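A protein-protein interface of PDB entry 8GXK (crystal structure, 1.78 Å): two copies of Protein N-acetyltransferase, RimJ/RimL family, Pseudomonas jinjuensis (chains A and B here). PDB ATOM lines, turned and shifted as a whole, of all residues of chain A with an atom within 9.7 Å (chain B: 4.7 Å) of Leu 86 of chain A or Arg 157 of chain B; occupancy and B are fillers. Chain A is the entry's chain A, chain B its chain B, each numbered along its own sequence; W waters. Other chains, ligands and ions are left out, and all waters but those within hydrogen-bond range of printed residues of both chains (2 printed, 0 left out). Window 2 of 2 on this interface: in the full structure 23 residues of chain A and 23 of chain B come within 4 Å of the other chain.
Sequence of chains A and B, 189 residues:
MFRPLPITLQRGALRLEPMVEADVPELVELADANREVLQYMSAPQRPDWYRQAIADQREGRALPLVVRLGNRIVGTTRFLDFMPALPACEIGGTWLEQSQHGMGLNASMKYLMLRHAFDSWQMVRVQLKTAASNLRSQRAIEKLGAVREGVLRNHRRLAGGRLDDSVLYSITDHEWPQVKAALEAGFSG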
ATOM      1  N   ASP A  81      34.001  33.223   9.712  1.00  0.00           N
ATOM      2  CA  ASP A  81      34.469  32.483   8.529  1.00  0.00           C
ATOM      3  C   ASP A  81      33.457  32.528   7.382  1.00  0.00           C
ATOM      4  O   ASP A  81      33.041  31.500   6.834  1.00  0.00           O
ATOM      5  CB  ASP A  81      34.812  31.040   8.912  1.00  0.00           C
ATOM      6  CG  ASP A  81      35.737  30.353   7.879  1.00  0.00           C
ATOM      7  OD1 ASP A  81      35.861  29.106   7.918  1.00  0.00           O
ATOM      8  OD2 ASP A  81      36.379  31.057   7.047  1.00  0.00           O
ATOM      9  N   PHE A  82      33.077  33.759   7.021  1.00  0.00           N
ATOM     10  CA  PHE A  82      32.117  33.991   5.957  1.00  0.00           C
ATOM     11  C   PHE A  82      32.802  33.749   4.628  1.00  0.00           C
ATOM     12  O   PHE A  82      33.921  34.210   4.402  1.00  0.00           O
ATOM     13  CB  PHE A  82      31.567  35.416   6.000  1.00  0.00           C
ATOM     14  CG  PHE A  82      30.654  35.688   7.165  1.00  0.00           C
ATOM     15  CD1 PHE A  82      31.133  36.336   8.290  1.00  0.00           C
ATOM     16  CD2 PHE A  82      29.319  35.280   7.145  1.00  0.00           C
ATOM     17  CE1 PHE A  82      30.304  36.572   9.355  1.00  0.00           C
ATOM     18  CE2 PHE A  82      28.483  35.533   8.219  1.00  0.00           C
ATOM     19  CZ  PHE A  82      28.972  36.178   9.305  1.00  0.00           C
ATOM     20  N   MET A  83      32.111  33.005   3.759  1.00  0.00           N
ATOM     21  CA  MET A  83      32.533  32.683   2.394  1.00  0.00           C
ATOM     22  C   MET A  83      31.489  33.278   1.454  1.00  0.00           C
ATOM     23  O   MET A  83      30.500  32.617   1.077  1.00  0.00           O
ATOM     24  CB  MET A  83      32.679  31.175   2.215  1.00  0.00           C
ATOM     25  CG  MET A  83      33.785  30.583   3.074  1.00  0.00           C
ATOM     26  SD  MET A  83      33.736  28.775   3.226  1.00  0.00           S
ATOM     27  CE  MET A  83      35.310  28.507   4.088  1.00  0.00           C
ATOM     28  N   PRO A  84      31.633  34.557   1.094  1.00  0.00           N
ATOM     29  CA  PRO A  84      30.512  35.267   0.448  1.00  0.00           C
ATOM     30  C   PRO A  84      30.116  34.735  -0.921  1.00  0.00           C
ATOM     31  O   PRO A  84      28.975  34.958  -1.341  1.00  0.00           O
ATOM     32  CB  PRO A  84      31.010  36.716   0.353  1.00  0.00           C
ATOM     33  CG  PRO A  84      32.263  36.764   1.211  1.00  0.00           C
ATOM     34  CD  PRO A  84      32.839  35.406   1.225  1.00  0.00           C
ATOM     35  N   ALA A  85      31.026  34.109  -1.657  1.00  0.00           N
ATOM     36  CA  ALA A  85      30.705  33.629  -2.995  1.00  0.00           C
ATOM     37  C   ALA A  85      29.759  32.447  -2.962  1.00  0.00           C
ATOM     38  O   ALA A  85      29.240  32.064  -4.016  1.00  0.00           O
ATOM     39  CB  ALA A  85      31.975  33.238  -3.741  1.00  0.00           C
ATOM     40  N   LEU A  86      29.527  31.843  -1.789  1.00  0.00           N
ATOM     41  CA  LEU A  86      28.791  30.582  -1.795  1.00  0.00           C
ATOM     42  C   LEU A  86      27.287  30.824  -1.609  1.00  0.00           C
ATOM     43  O   LEU A  86      26.489  30.429  -2.473  1.00  0.00           O
ATOM     44  CB  LEU A  86      29.369  29.624  -0.735  1.00  0.00           C
ATOM     45  CG  LEU A  86      30.853  29.254  -0.890  1.00  0.00           C
ATOM     46  CD1 LEU A  86      31.268  28.135   0.072  1.00  0.00           C
ATOM     47  CD2 LEU A  86      31.253  28.869  -2.301  1.00  0.00           C
ATOM     48  N   PRO A  87      26.841  31.467  -0.519  1.00  0.00           N
ATOM     49  CA  PRO A  87      27.552  31.963   0.667  1.00  0.00           C
ATOM     50  C   PRO A  87      27.544  30.888   1.734  1.00  0.00           C
ATOM     51  O   PRO A  87      26.615  30.042   1.764  1.00  0.00           O
ATOM     52  CB  PRO A  87      26.738  33.171   1.102  1.00  0.00           C
ATOM     53  CG  PRO A  87      25.340  32.823   0.664  1.00  0.00           C
ATOM     54  CD  PRO A  87      25.403  31.796  -0.471  1.00  0.00           C
ATOM     55  N   ALA A  88      28.540  30.941   2.611  1.00  0.00           N
ATOM     56  CA  ALA A  88      28.697  29.930   3.646  1.00  0.00           C
ATOM     57  C   ALA A  88      29.232  30.638   4.869  1.00  0.00           C
ATOM     58  O   ALA A  88      29.794  31.737   4.772  1.00  0.00           O
ATOM     59  CB  ALA A  88      29.631  28.782   3.242  1.00  0.00           C
ATOM     60  N   CYS A  89      29.055  30.013   6.031  1.00  0.00           N
ATOM     61  CA  CYS A  89      29.688  30.550   7.227  1.00  0.00           C
ATOM     62  C   CYS A  89      29.877  29.443   8.260  1.00  0.00           C
ATOM     63  O   CYS A  89      29.657  28.262   7.975  1.00  0.00           O
ATOM     64  CB  CYS A  89      28.884  31.722   7.789  1.00  0.00           C
ATOM     65  SG  CYS A  89      27.270  31.292   8.431  1.00  0.00           S
ATOM     66  N   GLU A  90      30.366  29.842   9.445  1.00  0.00           N
ATOM     67  CA  GLU A  90      30.589  28.984  10.605  1.00  0.00           C
ATOM     68  C   GLU A  90      29.844  29.538  11.812  1.00  0.00           C
ATOM     69  O   GLU A  90      29.706  30.752  11.950  1.00  0.00           O
ATOM     70  CB  GLU A  90      32.094  28.901  10.914  1.00  0.00           C
ATOM     71  CG  GLU A  90      32.460  28.009  12.069  1.00  0.00           C
ATOM     72  CD  GLU A  90      33.949  27.794  12.238  1.00  0.00           C
ATOM     73  OE1 GLU A  90      34.404  27.618  13.420  1.00  0.00           O
ATOM     74  OE2 GLU A  90      34.668  27.851  11.208  1.00  0.00           O
ATOM     75  N   ALA A 117      20.740  31.989   9.158  1.00  0.00           N
ATOM     76  CA  ALA A 117      21.719  31.737   8.106  1.00  0.00           C
ATOM     77  C   ALA A 117      21.070  31.142   6.859  1.00  0.00           C
ATOM     78  O   ALA A 117      21.389  31.532   5.731  1.00  0.00           O
ATOM     79  CB  ALA A 117      22.801  30.804   8.651  1.00  0.00           C
ATOM     80  N   TRP A 121      19.985  34.674   5.234  1.00  0.00           N
ATOM     81  CA  TRP A 121      21.201  34.839   4.453  1.00  0.00           C
ATOM     82  C   TRP A 121      21.313  33.905   3.260  1.00  0.00           C
ATOM     83  O   TRP A 121      22.284  34.015   2.503  1.00  0.00           O
ATOM     84  CB  TRP A 121      22.431  34.615   5.330  1.00  0.00           C
ATOM     85  CG  TRP A 121      22.631  35.675   6.356  1.00  0.00           C
ATOM     86  CD1 TRP A 121      22.088  36.913   6.349  1.00  0.00           C
ATOM     87  CD2 TRP A 121      23.455  35.606   7.511  1.00  0.00           C
ATOM     88  NE1 TRP A 121      22.514  37.627   7.437  1.00  0.00           N
ATOM     89  CE2 TRP A 121      23.322  36.826   8.191  1.00  0.00           C
ATOM     90  CE3 TRP A 121      24.229  34.602   8.084  1.00  0.00           C
ATOM     91  CZ2 TRP A 121      23.994  37.086   9.379  1.00  0.00           C
ATOM     92  CZ3 TRP A 121      24.882  34.854   9.262  1.00  0.00           C
ATOM     93  CH2 TRP A 121      24.774  36.080   9.897  1.00  0.00           C
ATOM     94  N   GLN A 122      20.404  32.946   3.127  1.00  0.00           N
ATOM     95  CA  GLN A 122      20.409  31.989   2.032  1.00  0.00           C
ATOM     96  C   GLN A 122      21.740  31.283   1.896  1.00  0.00           C
ATOM     97  O   GLN A 122      22.223  31.047   0.784  1.00  0.00           O
ATOM     98  CB  GLN A 122      20.025  32.685   0.737  1.00  0.00           C
ATOM     99  CG  GLN A 122      18.631  33.367   0.849  1.00  0.00           C
ATOM    100  CD  GLN A 122      17.528  32.387   0.476  1.00  0.00           C
ATOM    101  OE1 GLN A 122      17.195  32.236  -0.724  1.00  0.00           O
ATOM    102  NE2 GLN A 122      16.883  31.798   1.511  1.00  0.00           N
ATOM    103  N   MET A 123      22.298  30.895   3.045  1.00  0.00           N
ATOM    104  CA  MET A 123      23.526  30.121   3.074  1.00  0.00           C
ATOM    105  C   MET A 123      23.320  28.733   2.449  1.00  0.00           C
ATOM    106  O   MET A 123      22.270  28.091   2.587  1.00  0.00           O
ATOM    107  CB  MET A 123      24.043  30.014   4.527  1.00  0.00           C
ATOM    108  CG  MET A 123      24.447  31.321   5.196  1.00  0.00           C
ATOM    109  SD  MET A 123      26.052  31.900   4.673  1.00  0.00           S
ATOM    110  CE  MET A 123      26.278  33.486   5.542  1.00  0.00           C
ATOM    111  N   VAL A 124      24.382  28.270   1.795  1.00  0.00           N
ATOM    112  CA  VAL A 124      24.476  26.938   1.223  1.00  0.00           C
ATOM    113  C   VAL A 124      25.188  25.968   2.184  1.00  0.00           C
ATOM    114  O   VAL A 124      25.015  24.741   2.050  1.00  0.00           O
ATOM    115  CB  VAL A 124      25.172  27.139  -0.148  1.00  0.00           C
ATOM    116  CG1 VAL A 124      26.547  26.602  -0.154  1.00  0.00           C
ATOM    117  CG2 VAL A 124      24.265  26.803  -1.241  1.00  0.00           C
ATOM    118  N   ARG A 125      25.865  26.486   3.207  1.00  0.00           N
ATOM    119  CA  ARG A 125      26.650  25.660   4.115  1.00  0.00           C
ATOM    120  C   ARG A 125      26.866  26.465   5.392  1.00  0.00           C
ATOM    121  O   ARG A 125      27.248  27.640   5.324  1.00  0.00           O
ATOM    122  CB  ARG A 125      27.984  25.262   3.456  1.00  0.00           C
ATOM    123  CG  ARG A 125      29.054  24.714   4.389  1.00  0.00           C
ATOM    124  CD  ARG A 125      30.477  24.807   3.813  1.00  0.00           C
ATOM    125  NE  ARG A 125      31.448  24.287   4.797  1.00  0.00           N
ATOM    126  CZ  ARG A 125      31.696  23.005   5.034  1.00  0.00           C
ATOM    127  NH1 ARG A 125      32.566  22.693   5.982  1.00  0.00           N
ATOM    128  NH2 ARG A 125      31.061  22.062   4.344  1.00  0.00           N
ATOM    129  N   VAL A 126      26.589  25.838   6.534  1.00  0.00           N
ATOM    130  CA  VAL A 126      27.007  26.329   7.839  1.00  0.00           C
ATOM    131  C   VAL A 126      27.865  25.234   8.470  1.00  0.00           C
ATOM    132  O   VAL A 126      27.414  24.084   8.607  1.00  0.00           O
ATOM    133  CB  VAL A 126      25.817  26.683   8.752  1.00  0.00           C
ATOM    134  CG1 VAL A 126      26.375  27.157  10.096  1.00  0.00           C
ATOM    135  CG2 VAL A 126      24.956  27.791   8.142  1.00  0.00           C
ATOM    136  N   GLN A 127      29.095  25.570   8.839  1.00  0.00           N
ATOM    137  CA  GLN A 127      29.972  24.608   9.483  1.00  0.00           C
ATOM    138  C   GLN A 127      30.121  24.876  10.982  1.00  0.00           C
ATOM    139  O   GLN A 127      29.910  25.984  11.473  1.00  0.00           O
ATOM    140  CB  GLN A 127      31.340  24.577   8.779  1.00  0.00           C
ATOM    141  CG  GLN A 127      32.239  25.741   9.023  1.00  0.00           C
ATOM    142  CD  GLN A 127      33.565  25.613   8.294  1.00  0.00           C
ATOM    143  OE1 GLN A 127      33.699  24.932   7.283  1.00  0.00           O
ATOM    144  NE2 GLN A 127      34.539  26.294   8.801  1.00  0.00           N
ATOM    145  N   ASP A 173      22.180  23.647   2.819  1.00  0.00           N
ATOM    146  CA  ASP A 173      20.852  24.226   2.748  1.00  0.00           C
ATOM    147  C   ASP A 173      19.841  23.146   2.467  1.00  0.00           C
ATOM    148  O   ASP A 173      18.700  23.234   2.927  1.00  0.00           O
ATOM    149  CB  ASP A 173      20.759  25.302   1.684  1.00  0.00           C
ATOM    150  CG  ASP A 173      21.421  24.890   0.333  1.00  0.00           C
ATOM    151  OD1 ASP A 173      22.146  23.901   0.234  1.00  0.00           O
ATOM    152  OD2 ASP A 173      21.248  25.596  -0.663  1.00  0.00           O
ATOM    153  N   MET B  41      39.226  25.667 -10.710  1.00  0.00           N
ATOM    154  CA  MET B  41      39.566  26.680  -9.721  1.00  0.00           C
ATOM    155  C   MET B  41      38.528  27.780  -9.781  1.00  0.00           C
ATOM    156  O   MET B  41      37.882  27.983 -10.803  1.00  0.00           O
ATOM    157  CB  MET B  41      40.959  27.259  -9.949  1.00  0.00           C
ATOM    158  CG  MET B  41      42.039  26.193  -9.894  1.00  0.00           C
ATOM    159  SD  MET B  41      43.673  26.928 -10.139  1.00  0.00           S
ATOM    160  CE  MET B  41      43.969  27.759  -8.548  1.00  0.00           C
ATOM    161  N   SER B  42      38.358  28.485  -8.683  1.00  0.00           N
ATOM    162  CA  SER B  42      37.517  29.678  -8.644  1.00  0.00           C
ATOM    163  C   SER B  42      38.441  30.880  -8.801  1.00  0.00           C
ATOM    164  O   SER B  42      39.204  31.210  -7.892  1.00  0.00           O
ATOM    165  CB  SER B  42      36.769  29.764  -7.324  1.00  0.00           C
ATOM    166  OG  SER B  42      37.700  30.166  -6.330  1.00  0.00           O
ATOM    167  N   ASN B 154      29.374  21.542  -0.332  1.00  0.00           N
ATOM    168  CA  ASN B 154      28.903  22.885  -0.720  1.00  0.00           C
ATOM    169  C   ASN B 154      29.908  23.964  -0.290  1.00  0.00           C
ATOM    170  O   ASN B 154      29.552  24.961   0.345  1.00  0.00           O
ATOM    171  CB  ASN B 154      27.537  23.198  -0.113  1.00  0.00           C
ATOM    172  CG  ASN B 154      26.412  22.429  -0.727  1.00  0.00           C
ATOM    173  OD1 ASN B 154      26.616  21.552  -1.610  1.00  0.00           O
ATOM    174  ND2 ASN B 154      25.167  22.764  -0.272  1.00  0.00           N
ATOM    175  N   HIS B 155      31.180  23.764  -0.650  1.00  0.00           N
ATOM    176  CA  HIS B 155      32.318  24.480  -0.067  1.00  0.00           C
ATOM    177  C   HIS B 155      33.110  25.341  -1.063  1.00  0.00           C
ATOM    178  O   HIS B 155      34.055  26.042  -0.651  1.00  0.00           O
ATOM    179  CB  HIS B 155      33.260  23.449   0.588  1.00  0.00           C
ATOM    180  CG  HIS B 155      34.344  24.069   1.402  1.00  0.00           C
ATOM    181  ND1 HIS B 155      35.656  24.115   0.986  1.00  0.00           N
ATOM    182  CD2 HIS B 155      34.303  24.700   2.600  1.00  0.00           C
ATOM    183  CE1 HIS B 155      36.370  24.774   1.879  1.00  0.00           C
ATOM    184  NE2 HIS B 155      35.569  25.162   2.856  1.00  0.00           N
ATOM    185  N   ARG B 156      32.785  25.286  -2.348  1.00  0.00           N
ATOM    186  CA  ARG B 156      33.541  26.051  -3.325  1.00  0.00           C
ATOM    187  C   ARG B 156      32.686  26.217  -4.573  1.00  0.00           C
ATOM    188  O   ARG B 156      31.688  25.512  -4.763  1.00  0.00           O
ATOM    189  CB  ARG B 156      34.865  25.359  -3.670  1.00  0.00           C
ATOM    190  CG  ARG B 156      34.629  24.059  -4.401  1.00  0.00           C
ATOM    191  CD  ARG B 156      35.883  23.388  -4.889  1.00  0.00           C
ATOM    192  NE  ARG B 156      36.861  23.256  -3.831  1.00  0.00           N
ATOM    193  CZ  ARG B 156      38.046  23.864  -3.817  1.00  0.00           C
ATOM    194  NH1 ARG B 156      38.469  24.631  -4.823  1.00  0.00           N
ATOM    195  NH2 ARG B 156      38.817  23.665  -2.778  1.00  0.00           N
ATOM    196  N   ARG B 157      33.134  27.097  -5.460  1.00  0.00           N
ATOM    197  CA  ARG B 157      32.561  27.181  -6.791  1.00  0.00           C
ATOM    198  C   ARG B 157      33.664  26.933  -7.789  1.00  0.00           C
ATOM    199  O   ARG B 157      34.806  27.348  -7.576  1.00  0.00           O
ATOM    200  CB  ARG B 157      31.895  28.531  -7.050  1.00  0.00           C
ATOM    201  CG  ARG B 157      30.602  28.671  -6.242  1.00  0.00           C
ATOM    202  CD  ARG B 157      29.774  29.892  -6.669  1.00  0.00           C
ATOM    203  NE  ARG B 157      28.617  29.933  -5.791  1.00  0.00           N
ATOM    204  CZ  ARG B 157      27.502  29.253  -6.004  1.00  0.00           C
ATOM    205  NH1 ARG B 157      27.359  28.465  -7.067  1.00  0.00           N
ATOM    206  NH2 ARG B 157      26.532  29.325  -5.126  1.00  0.00           N
ATOM    207  N   LEU B 158      33.310  26.225  -8.859  1.00  0.00           N
ATOM    208  CA  LEU B 158      34.203  25.976  -9.971  1.00  0.00           C
ATOM    209  C   LEU B 158      34.315  27.234 -10.820  1.00  0.00           C
ATOM    210  O   LEU B 158      33.651  28.239 -10.579  1.00  0.00           O
ATOM    211  CB  LEU B 158      33.696  24.803 -10.782  1.00  0.00           C
ATOM    212  CG  LEU B 158      33.563  23.555  -9.924  1.00  0.00           C
ATOM    213  CD1 LEU B 158      33.086  22.309 -10.731  1.00  0.00           C
ATOM    214  CD2 LEU B 158      34.805  23.210  -9.176  1.00  0.00           C
ATOM    215  N   ALA B 159      35.179  27.195 -11.830  1.00  0.00           N
ATOM    216  CA  ALA B 159      35.492  28.411 -12.568  1.00  0.00           C
ATOM    217  C   ALA B 159      34.241  29.063 -13.139  1.00  0.00           C
ATOM    218  O   ALA B 159      34.097  30.290 -13.082  1.00  0.00           O
ATOM    219  CB  ALA B 159      36.481  28.095 -13.689  1.00  0.00           C
ATOM    220  N   GLY B 161      31.173  28.780 -12.090  1.00  0.00           N
ATOM    221  CA  GLY B 161      30.139  29.104 -11.129  1.00  0.00           C
ATOM    222  C   GLY B 161      29.516  27.939 -10.401  1.00  0.00           C
ATOM    223  O   GLY B 161      28.755  28.174  -9.448  1.00  0.00           O
ATOM    224  N   ARG B 162      29.773  26.698 -10.821  1.00  0.00           N
ATOM    225  CA  ARG B 162      29.032  25.575 -10.270  1.00  0.00           C
ATOM    226  C   ARG B 162      29.537  25.228  -8.876  1.00  0.00           C
ATOM    227  O   ARG B 162      30.741  25.259  -8.609  1.00  0.00           O
ATOM    228  CB  ARG B 162      29.122  24.348 -11.172  1.00  0.00           C
ATOM    229  CG  ARG B 162      28.345  23.154 -10.638  1.00  0.00           C
ATOM    230  CD  ARG B 162      27.521  22.502 -11.750  1.00  0.00           C
ATOM    231  NE  ARG B 162      26.724  21.393 -11.232  1.00  0.00           N
ATOM    232  CZ  ARG B 162      26.026  20.578 -12.003  1.00  0.00           C
ATOM    233  NH1 ARG B 162      25.328  19.580 -11.464  1.00  0.00           N
ATOM    234  NH2 ARG B 162      26.027  20.779 -13.321  1.00  0.00           N
ATOM    235  N   LEU B 163      28.595  24.955  -7.986  1.00  0.00           N
ATOM    236  CA  LEU B 163      28.924  24.569  -6.624  1.00  0.00           C
ATOM    237  C   LEU B 163      29.532  23.179  -6.638  1.00  0.00           C
ATOM    238  O   LEU B 163      29.080  22.292  -7.365  1.00  0.00           O
ATOM    239  CB  LEU B 163      27.658  24.552  -5.762  1.00  0.00           C
ATOM    240  CG  LEU B 163      27.279  25.413  -4.578  1.00  0.00           C
ATOM    241  CD1 LEU B 163      26.231  24.616  -3.714  1.00  0.00           C
ATOM    242  CD2 LEU B 163      28.460  25.849  -3.806  1.00  0.00           C
HETATM  243  O   HOH W   1      23.954  30.313  -3.474  1.00  0.00           O
HETATM  244  O   HOH W   2      35.599  25.663   5.515  1.00  0.00           O
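Leu 86 of chain A touches four residues of chain B.
Gln 127 of chain A touches none of the printed residues of chain B.
Of the printed residues of chain A, His 155 of chain B touches Met 83, Leu 86 and Arg 125.
Arg 157 of chain B touches two residues of chain A.
No residue of chain A comes within 4 Å of Leu 158 of chain B.
No residue of chain A comes within 4 Å of Gly 161 of chain B.
Printed residues of chain A within 4 Å of Leu 163 of chain B: Val 124 (3.8 Å).
The nearest residue of chain B that does not touch Leu 86 of chain A is Leu 163 of chain B (4.4 Å).
The nearest residue of chain A that does not touch Arg 157 of chain B is Pro 87 of chain A (5.1 Å).
The nearest printed residue of chain B that does not touch Ala 85 of chain A is Leu 163 of chain B (6.3 Å).
The backbone carbonyl oxygen (O) of Val 124 of chain A sits at hydrogen-bond distance from the side-chain amide nitrogen (ND2) of Asn 154 of chain B.
NE of Arg 157 of chain B lies within hydrogen-bond range of O of Ala 85 of chain A (2.8 Å).
The guanidinium group (NH2) of Arg 157 of chain B lies within hydrogen-bond range of the backbone carbonyl oxygen (O) of Leu 86 of chain A (2.9 Å).
The side-chain amide nitrogen (ND2) of Asn 154 of chain B is in hydrogen-bond range of the side-chain carboxylate (OD1) of Asp 173 of chain A (3.3 Å).
No position is printed for both chains.
Of the 19 printed residues of chain A, 6 touch a printed residue of chain B.
Hydrophobic or aromatic side chains of chain A that line the printed part of chain B: Met 83, Leu 86 and Val 124.
Among the printed residues, 11 pairs touch across the chains.
Among the printed residues, no Asp or Glu carboxylate lies within 4 Å of a Lys or Arg side-chain nitrogen of the other chain.
Water W2 lies within hydrogen-bond range of OE1 of Gln 127 of chain A and NE2 of His 155 of chain B.
Water W1 bridges O of Leu 86 of chain A (2.7 Å) and NH2 of Arg 157 of chain B (3.2 Å).
The guanidinium group of Arg 125 of chain A lies within hydrogen-bond range of the side-chain amide oxygen of Gln 127 of chain A.
The backbone NH of Met 83 of chain A sits at hydrogen-bond distance from the backbone carbonyl oxygen of Ala 88 of chain A, at 2.8 Å.
The backbone NH (N) of Val 124 of chain A sits at hydrogen-bond distance from the backbone carbonyl oxygen (O) of Pro 87 of chain A, at 2.9 Å.
The backbone NH (N) of Cys 89 of chain A sits at hydrogen-bond distance from the backbone carbonyl oxygen (O) of Arg 125 of chain A, at 3.1 Å.
The backbone carbonyl oxygen (O) of Val 124 of chain A is in hydrogen-bond range of the backbone NH (N) of Asp 173 of chain A, at 3.1 Å.
The guanidinium group (NH1) of Arg 157 of chain B sits at hydrogen-bond distance from the backbone carbonyl oxygen (O) of Gly 161 of chain B, at 2.8 Å.
CE of Met 83 of chain A touches NE2 of His 155 of chain B, 3.6 Å away.
Asn 154 of chain B touches Leu 86 of chain A (O to CD1, 3.6 Å).
Leu 86 of chain A touches His 155 of chain B (CD1 to C, 3.5 Å).
Leu 86 of chain A touches Arg 156 of chain B (CD2 to CA, 3.8 Å).
Leu 163 of chain B touches Val 124 of chain A (CD1 to CG2, 3.8 Å).
CB of Arg 125 of chain A touches O of Asn 154 of chain B, at 3.5 Å.
NE of Arg 125 of chain A touches CD2 of His 155 of chain B, at 3.6 Å.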
